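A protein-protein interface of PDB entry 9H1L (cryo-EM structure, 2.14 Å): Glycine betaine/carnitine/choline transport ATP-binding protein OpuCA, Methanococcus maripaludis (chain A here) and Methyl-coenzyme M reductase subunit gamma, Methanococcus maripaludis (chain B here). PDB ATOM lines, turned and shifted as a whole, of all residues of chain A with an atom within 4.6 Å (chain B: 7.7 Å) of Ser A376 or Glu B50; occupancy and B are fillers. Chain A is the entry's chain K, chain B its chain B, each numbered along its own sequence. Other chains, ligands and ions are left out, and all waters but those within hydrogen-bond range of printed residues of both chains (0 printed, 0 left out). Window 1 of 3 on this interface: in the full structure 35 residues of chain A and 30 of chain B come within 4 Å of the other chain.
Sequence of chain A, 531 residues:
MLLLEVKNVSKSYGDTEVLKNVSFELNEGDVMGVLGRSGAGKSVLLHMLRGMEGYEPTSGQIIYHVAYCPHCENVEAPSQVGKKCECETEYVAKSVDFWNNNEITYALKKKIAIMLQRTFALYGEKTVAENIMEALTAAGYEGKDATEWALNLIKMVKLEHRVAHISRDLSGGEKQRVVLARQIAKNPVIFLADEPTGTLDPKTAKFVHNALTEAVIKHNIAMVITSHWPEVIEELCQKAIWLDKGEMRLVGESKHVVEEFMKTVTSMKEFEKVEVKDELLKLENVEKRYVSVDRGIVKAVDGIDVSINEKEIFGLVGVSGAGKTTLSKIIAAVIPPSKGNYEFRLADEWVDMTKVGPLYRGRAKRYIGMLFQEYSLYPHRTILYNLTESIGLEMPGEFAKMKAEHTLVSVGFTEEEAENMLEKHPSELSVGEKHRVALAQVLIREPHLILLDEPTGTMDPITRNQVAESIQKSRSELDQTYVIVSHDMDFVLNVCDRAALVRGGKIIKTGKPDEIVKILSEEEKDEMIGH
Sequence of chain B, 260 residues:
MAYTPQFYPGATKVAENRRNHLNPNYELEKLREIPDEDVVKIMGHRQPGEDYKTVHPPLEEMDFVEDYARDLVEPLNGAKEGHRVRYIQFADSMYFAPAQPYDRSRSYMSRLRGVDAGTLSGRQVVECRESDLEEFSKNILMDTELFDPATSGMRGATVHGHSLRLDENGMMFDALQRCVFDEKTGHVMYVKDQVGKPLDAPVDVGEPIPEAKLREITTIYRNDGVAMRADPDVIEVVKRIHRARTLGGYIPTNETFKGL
Printed residues of chain B that touch a printed residue of chain A: Arg B46, Gln B47, Pro B48, Gly B49, Glu B50 and Asp B51. Hydrophobic or aromatic side chains of chain A within 4 Å of the printed part of chain B: Phe A372 and Tyr A375. Among the printed residues, no Asp or Glu carboxylate lies within 4 Å of a Lys or Arg side-chain nitrogen of the other chain.
Among the printed residues, merely in contact across the chains: Phe A372 with Gln B47, Phe A372 with Pro B48, Phe A372 with Gly B49, Phe A372 with Glu B50, Glu A374 with Glu B50, Tyr A375 with Gly B49, Tyr A375 with Asp B51 and Ser A376 with Asp B51.
NH1 of Arg B46 is in salt-bridge range of OE1 of Glu B134, at 3.0 Å. NH2 of Arg B46 sits at hydrogen-bond distance from O of Glu B50 (2.9 Å). The guanidinium group of Arg B46 is in hydrogen-bond range of the side-chain hydroxyl of Tyr B52 (3.3 Å).
Printed residues of chain B within 4 Å of Glu A374: Glu B50 and Asp B51. Of the printed residues of chain B, Tyr A375 touches Gly B49 (3.4 Å) and Asp B51 (3.4 Å). Leu A377 touches none of the printed residues of chain B. Of the printed residues of chain A, Arg B46 touches Ser A376. Printed residues of chain A within 4 Å of Gly B49: Phe A372 (3.6 Å), Tyr A375 (3.4 Å) and Ser A376 (3.2 Å). Of the printed residues of chain A, Glu B50 touches Phe A372, Glu A374 and Ser A376. Of the printed residues of chain A, Asp B51 touches Glu A374 (2.6 Å), Tyr A375 (3.4 Å) and Ser A376 (3.4 Å). Arg B84 touches none of the printed residues of chain A. The nearest residue of chain B that does not touch Ser A376 is Tyr B52 (4.5 Å).
The backbone carbonyl oxygen (O) of Gly B49 is in hydrogen-bond range of the backbone NH (N) of Ser A376, at 3.2 Å. The guanidinium group (NH2) of Arg B46 is in hydrogen-bond range of the side-chain hydroxyl (OG) of Ser A376 (3.3 Å). The backbone carbonyl oxygen (O) of Glu A374 sits at hydrogen-bond distance from the backbone NH (N) of Asp B51. O of Glu B50 is in hydrogen-bond range of OG of Ser A376 (2.4 Å).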
ATOM      1  N   LYS A 329      -7.668  -8.543  15.932  1.00  0.00           N
ATOM      2  CA  LYS A 329      -7.012  -9.340  16.959  1.00  0.00           C
ATOM      3  C   LYS A 329      -7.382 -10.811  16.844  1.00  0.00           C
ATOM      4  O   LYS A 329      -6.580 -11.680  17.204  1.00  0.00           O
ATOM      5  CB  LYS A 329      -7.365  -8.807  18.346  1.00  0.00           C
ATOM      6  CG  LYS A 329      -6.550  -7.601  18.764  1.00  0.00           C
ATOM      7  CD  LYS A 329      -7.005  -7.066  20.106  1.00  0.00           C
ATOM      8  CE  LYS A 329      -6.139  -5.901  20.550  1.00  0.00           C
ATOM      9  NZ  LYS A 329      -6.565  -5.367  21.870  1.00  0.00           N
ATOM     10  N   PHE A 372      -0.680  -2.646  16.306  1.00  0.00           N
ATOM     11  CA  PHE A 372      -1.869  -2.374  17.093  1.00  0.00           C
ATOM     12  C   PHE A 372      -2.281  -0.912  16.970  1.00  0.00           C
ATOM     13  O   PHE A 372      -1.468  -0.030  16.683  1.00  0.00           O
ATOM     14  CB  PHE A 372      -1.631  -2.730  18.560  1.00  0.00           C
ATOM     15  CG  PHE A 372      -1.483  -4.200  18.806  1.00  0.00           C
ATOM     16  CD1 PHE A 372      -0.244  -4.810  18.705  1.00  0.00           C
ATOM     17  CD2 PHE A 372      -2.580  -4.975  19.131  1.00  0.00           C
ATOM     18  CE1 PHE A 372      -0.103  -6.164  18.926  1.00  0.00           C
ATOM     19  CE2 PHE A 372      -2.447  -6.330  19.353  1.00  0.00           C
ATOM     20  CZ  PHE A 372      -1.207  -6.924  19.248  1.00  0.00           C
ATOM     21  N   GLU A 374      -3.439   0.805  19.542  1.00  0.00           N
ATOM     22  CA  GLU A 374      -2.738   1.346  20.704  1.00  0.00           C
ATOM     23  C   GLU A 374      -1.366   0.678  20.763  1.00  0.00           C
ATOM     24  O   GLU A 374      -1.124  -0.264  21.513  1.00  0.00           O
ATOM     25  CB  GLU A 374      -3.544   1.117  21.977  1.00  0.00           C
ATOM     26  CG  GLU A 374      -4.831   1.920  22.041  1.00  0.00           C
ATOM     27  CD  GLU A 374      -6.017   1.084  22.475  1.00  0.00           C
ATOM     28  OE1 GLU A 374      -6.264   0.982  23.695  1.00  0.00           O
ATOM     29  OE2 GLU A 374      -6.708   0.528  21.596  1.00  0.00           O
ATOM     30  N   TYR A 375      -0.456   1.190  19.939  1.00  0.00           N
ATOM     31  CA  TYR A 375       0.879   0.639  19.790  1.00  0.00           C
ATOM     32  C   TYR A 375       1.795   1.125  20.910  1.00  0.00           C
ATOM     33  O   TYR A 375       1.482   2.062  21.648  1.00  0.00           O
ATOM     34  CB  TYR A 375       1.458   1.016  18.422  1.00  0.00           C
ATOM     35  CG  TYR A 375       1.652   2.508  18.214  1.00  0.00           C
ATOM     36  CD1 TYR A 375       0.608   3.306  17.763  1.00  0.00           C
ATOM     37  CD2 TYR A 375       2.877   3.115  18.466  1.00  0.00           C
ATOM     38  CE1 TYR A 375       0.777   4.664  17.575  1.00  0.00           C
ATOM     39  CE2 TYR A 375       3.054   4.471  18.282  1.00  0.00           C
ATOM     40  CZ  TYR A 375       2.002   5.241  17.834  1.00  0.00           C
ATOM     41  OH  TYR A 375       2.173   6.591  17.647  1.00  0.00           O
ATOM     42  N   SER A 376       2.951   0.473  21.026  1.00  0.00           N
ATOM     43  CA  SER A 376       3.998   0.931  21.926  1.00  0.00           C
ATOM     44  C   SER A 376       5.340   0.419  21.436  1.00  0.00           C
ATOM     45  O   SER A 376       5.422  -0.531  20.655  1.00  0.00           O
ATOM     46  CB  SER A 376       3.770   0.467  23.367  1.00  0.00           C
ATOM     47  OG  SER A 376       3.620  -0.939  23.428  1.00  0.00           O
ATOM     48  N   LEU A 377       6.393   1.064  21.912  1.00  0.00           N
ATOM     49  CA  LEU A 377       7.768   0.638  21.713  1.00  0.00           C
ATOM     50  C   LEU A 377       8.372   0.333  23.081  1.00  0.00           C
ATOM     51  O   LEU A 377       7.673   0.298  24.097  1.00  0.00           O
ATOM     52  CB  LEU A 377       8.562   1.708  20.965  1.00  0.00           C
ATOM     53  CG  LEU A 377       8.008   2.161  19.613  1.00  0.00           C
ATOM     54  CD1 LEU A 377       8.684   3.444  19.172  1.00  0.00           C
ATOM     55  CD2 LEU A 377       8.191   1.071  18.573  1.00  0.00           C
ATOM     56  N   VAL B  40       8.650 -10.469  27.460  1.00  0.00           N
ATOM     57  CA  VAL B  40       7.259 -10.053  27.638  1.00  0.00           C
ATOM     58  C   VAL B  40       6.314 -11.241  27.458  1.00  0.00           C
ATOM     59  O   VAL B  40       5.349 -11.407  28.216  1.00  0.00           O
ATOM     60  CB  VAL B  40       6.930  -8.893  26.679  1.00  0.00           C
ATOM     61  CG1 VAL B  40       5.433  -8.667  26.564  1.00  0.00           C
ATOM     62  CG2 VAL B  40       7.617  -7.620  27.140  1.00  0.00           C
ATOM     63  N   HIS B  45       1.994 -10.819  30.821  1.00  0.00           N
ATOM     64  CA  HIS B  45       1.137  -9.738  31.294  1.00  0.00           C
ATOM     65  C   HIS B  45       0.461  -9.013  30.137  1.00  0.00           C
ATOM     66  O   HIS B  45      -0.747  -8.758  30.178  1.00  0.00           O
ATOM     67  CB  HIS B  45       1.950  -8.758  32.138  1.00  0.00           C
ATOM     68  CG  HIS B  45       2.503  -9.355  33.392  1.00  0.00           C
ATOM     69  ND1 HIS B  45       1.777 -10.213  34.190  1.00  0.00           N
ATOM     70  CD2 HIS B  45       3.712  -9.221  33.986  1.00  0.00           C
ATOM     71  CE1 HIS B  45       2.513 -10.579  35.221  1.00  0.00           C
ATOM     72  NE2 HIS B  45       3.692  -9.992  35.123  1.00  0.00           N
ATOM     73  N   ARG B  46       1.220  -8.677  29.096  1.00  0.00           N
ATOM     74  CA  ARG B  46       0.698  -7.897  27.988  1.00  0.00           C
ATOM     75  C   ARG B  46       1.149  -8.504  26.670  1.00  0.00           C
ATOM     76  O   ARG B  46       2.159  -9.208  26.596  1.00  0.00           O
ATOM     77  CB  ARG B  46       1.153  -6.435  28.065  1.00  0.00           C
ATOM     78  CG  ARG B  46       2.654  -6.263  28.151  1.00  0.00           C
ATOM     79  CD  ARG B  46       3.060  -4.820  27.929  1.00  0.00           C
ATOM     80  NE  ARG B  46       3.184  -4.495  26.516  1.00  0.00           N
ATOM     81  CZ  ARG B  46       4.336  -4.256  25.902  1.00  0.00           C
ATOM     82  NH1 ARG B  46       5.486  -4.312  26.548  1.00  0.00           N
ATOM     83  NH2 ARG B  46       4.330  -3.956  24.607  1.00  0.00           N
ATOM     84  N   GLN B  47       0.375  -8.231  25.633  1.00  0.00           N
ATOM     85  CA  GLN B  47       0.769  -8.605  24.284  1.00  0.00           C
ATOM     86  C   GLN B  47       1.905  -7.701  23.820  1.00  0.00           C
ATOM     87  O   GLN B  47       1.820  -6.479  23.982  1.00  0.00           O
ATOM     88  CB  GLN B  47      -0.425  -8.492  23.340  1.00  0.00           C
ATOM     89  CG  GLN B  47      -0.094  -8.699  21.878  1.00  0.00           C
ATOM     90  CD  GLN B  47       0.267 -10.133  21.560  1.00  0.00           C
ATOM     91  OE1 GLN B  47       1.188 -10.396  20.788  1.00  0.00           O
ATOM     92  NE2 GLN B  47      -0.462 -11.070  22.152  1.00  0.00           N
ATOM     93  N   PRO B  48       2.992  -8.254  23.279  1.00  0.00           N
ATOM     94  CA  PRO B  48       4.064  -7.398  22.759  1.00  0.00           C
ATOM     95  C   PRO B  48       3.604  -6.605  21.544  1.00  0.00           C
ATOM     96  O   PRO B  48       2.935  -7.129  20.653  1.00  0.00           O
ATOM     97  CB  PRO B  48       5.173  -8.394  22.395  1.00  0.00           C
ATOM     98  CG  PRO B  48       4.491  -9.709  22.271  1.00  0.00           C
ATOM     99  CD  PRO B  48       3.346  -9.681  23.229  1.00  0.00           C
ATOM    100  N   GLY B  49       3.974  -5.327  21.521  1.00  0.00           N
ATOM    101  CA  GLY B  49       3.592  -4.419  20.469  1.00  0.00           C
ATOM    102  C   GLY B  49       2.412  -3.527  20.795  1.00  0.00           C
ATOM    103  O   GLY B  49       2.236  -2.501  20.132  1.00  0.00           O
ATOM    104  N   GLU B  50       1.609  -3.882  21.791  1.00  0.00           N
ATOM    105  CA  GLU B  50       0.482  -3.063  22.207  1.00  0.00           C
ATOM    106  C   GLU B  50       0.873  -2.195  23.397  1.00  0.00           C
ATOM    107  O   GLU B  50       1.850  -2.465  24.100  1.00  0.00           O
ATOM    108  CB  GLU B  50      -0.731  -3.931  22.551  1.00  0.00           C
ATOM    109  CG  GLU B  50      -0.751  -4.463  23.969  1.00  0.00           C
ATOM    110  CD  GLU B  50      -2.017  -5.236  24.282  1.00  0.00           C
ATOM    111  OE1 GLU B  50      -2.845  -5.420  23.365  1.00  0.00           O
ATOM    112  OE2 GLU B  50      -2.180  -5.662  25.447  1.00  0.00           O
ATOM    113  N   ASP B  51       0.104  -1.129  23.602  1.00  0.00           N
ATOM    114  CA  ASP B  51       0.452  -0.139  24.608  1.00  0.00           C
ATOM    115  C   ASP B  51       0.205  -0.669  26.016  1.00  0.00           C
ATOM    116  O   ASP B  51      -0.594  -1.583  26.241  1.00  0.00           O
ATOM    117  CB  ASP B  51      -0.342   1.149  24.392  1.00  0.00           C
ATOM    118  CG  ASP B  51       0.430   2.383  24.813  1.00  0.00           C
ATOM    119  OD1 ASP B  51       1.590   2.243  25.256  1.00  0.00           O
ATOM    120  OD2 ASP B  51      -0.122   3.497  24.701  1.00  0.00           O
ATOM    121  N   TYR B  52       0.922  -0.084  26.973  1.00  0.00           N
ATOM    122  CA  TYR B  52       0.757  -0.452  28.370  1.00  0.00           C
ATOM    123  C   TYR B  52      -0.579   0.049  28.900  1.00  0.00           C
ATOM    124  O   TYR B  52      -0.969   1.196  28.665  1.00  0.00           O
ATOM    125  CB  TYR B  52       1.894   0.124  29.212  1.00  0.00           C
ATOM    126  CG  TYR B  52       3.273  -0.344  28.815  1.00  0.00           C
ATOM    127  CD1 TYR B  52       3.793  -1.529  29.320  1.00  0.00           C
ATOM    128  CD2 TYR B  52       4.060   0.401  27.949  1.00  0.00           C
ATOM    129  CE1 TYR B  52       5.053  -1.960  28.966  1.00  0.00           C
ATOM    130  CE2 TYR B  52       5.323  -0.024  27.589  1.00  0.00           C
ATOM    131  CZ  TYR B  52       5.814  -1.206  28.101  1.00  0.00           C
ATOM    132  OH  TYR B  52       7.071  -1.635  27.747  1.00  0.00           O
ATOM    133  N   LYS B  53      -1.284  -0.821  29.617  1.00  0.00           N
ATOM    134  CA  LYS B  53      -2.509  -0.413  30.285  1.00  0.00           C
ATOM    135  C   LYS B  53      -2.188   0.514  31.452  1.00  0.00           C
ATOM    136  O   LYS B  53      -1.156   0.383  32.113  1.00  0.00           O
ATOM    137  CB  LYS B  53      -3.285  -1.632  30.778  1.00  0.00           C
ATOM    138  CG  LYS B  53      -3.589  -2.650  29.696  1.00  0.00           C
ATOM    139  CD  LYS B  53      -4.251  -3.887  30.272  1.00  0.00           C
ATOM    140  CE  LYS B  53      -5.495  -4.264  29.486  1.00  0.00           C
ATOM    141  NZ  LYS B  53      -5.391  -3.869  28.054  1.00  0.00           N
ATOM    142  N   ARG B  84       0.108   0.067  35.214  1.00  0.00           N
ATOM    143  CA  ARG B  84      -0.262  -0.891  36.240  1.00  0.00           C
ATOM    144  C   ARG B  84       0.982  -1.573  36.798  1.00  0.00           C
ATOM    145  O   ARG B  84       2.008  -1.698  36.125  1.00  0.00           O
ATOM    146  CB  ARG B  84      -1.244  -1.922  35.684  1.00  0.00           C
ATOM    147  CG  ARG B  84      -0.638  -2.930  34.734  1.00  0.00           C
ATOM    148  CD  ARG B  84      -1.622  -3.318  33.653  1.00  0.00           C
ATOM    149  NE  ARG B  84      -1.031  -4.239  32.691  1.00  0.00           N
ATOM    150  CZ  ARG B  84      -1.502  -5.449  32.431  1.00  0.00           C
ATOM    151  NH1 ARG B  84      -2.585  -5.912  33.033  1.00  0.00           N
ATOM    152  NH2 ARG B  84      -0.876  -6.211  31.540  1.00  0.00           N
ATOM    153  N   GLU B 130       5.034  -1.614  34.954  1.00  0.00           N
ATOM    154  CA  GLU B 130       5.192  -2.654  33.937  1.00  0.00           C
ATOM    155  C   GLU B 130       6.372  -2.390  33.005  1.00  0.00           C
ATOM    156  O   GLU B 130       7.119  -3.317  32.669  1.00  0.00           O
ATOM    157  CB  GLU B 130       3.896  -2.783  33.138  1.00  0.00           C
ATOM    158  CG  GLU B 130       3.875  -3.935  32.153  1.00  0.00           C
ATOM    159  CD  GLU B 130       2.472  -4.301  31.725  1.00  0.00           C
ATOM    160  OE1 GLU B 130       1.749  -3.412  31.225  1.00  0.00           O
ATOM    161  OE2 GLU B 130       2.086  -5.476  31.882  1.00  0.00           O
ATOM    162  N   GLU B 134       9.671  -4.677  33.041  1.00  0.00           N
ATOM    163  CA  GLU B 134      10.167  -5.353  31.847  1.00  0.00           C
ATOM    164  C   GLU B 134      11.619  -4.991  31.567  1.00  0.00           C
ATOM    165  O   GLU B 134      12.413  -5.851  31.158  1.00  0.00           O
ATOM    166  CB  GLU B 134       9.290  -5.004  30.647  1.00  0.00           C
ATOM    167  CG  GLU B 134       8.008  -5.810  30.562  1.00  0.00           C
ATOM    168  CD  GLU B 134       6.971  -5.165  29.671  1.00  0.00           C
ATOM    169  OE1 GLU B 134       7.343  -4.296  28.853  1.00  0.00           O
ATOM    170  OE2 GLU B 134       5.780  -5.524  29.785  1.00  0.00           O
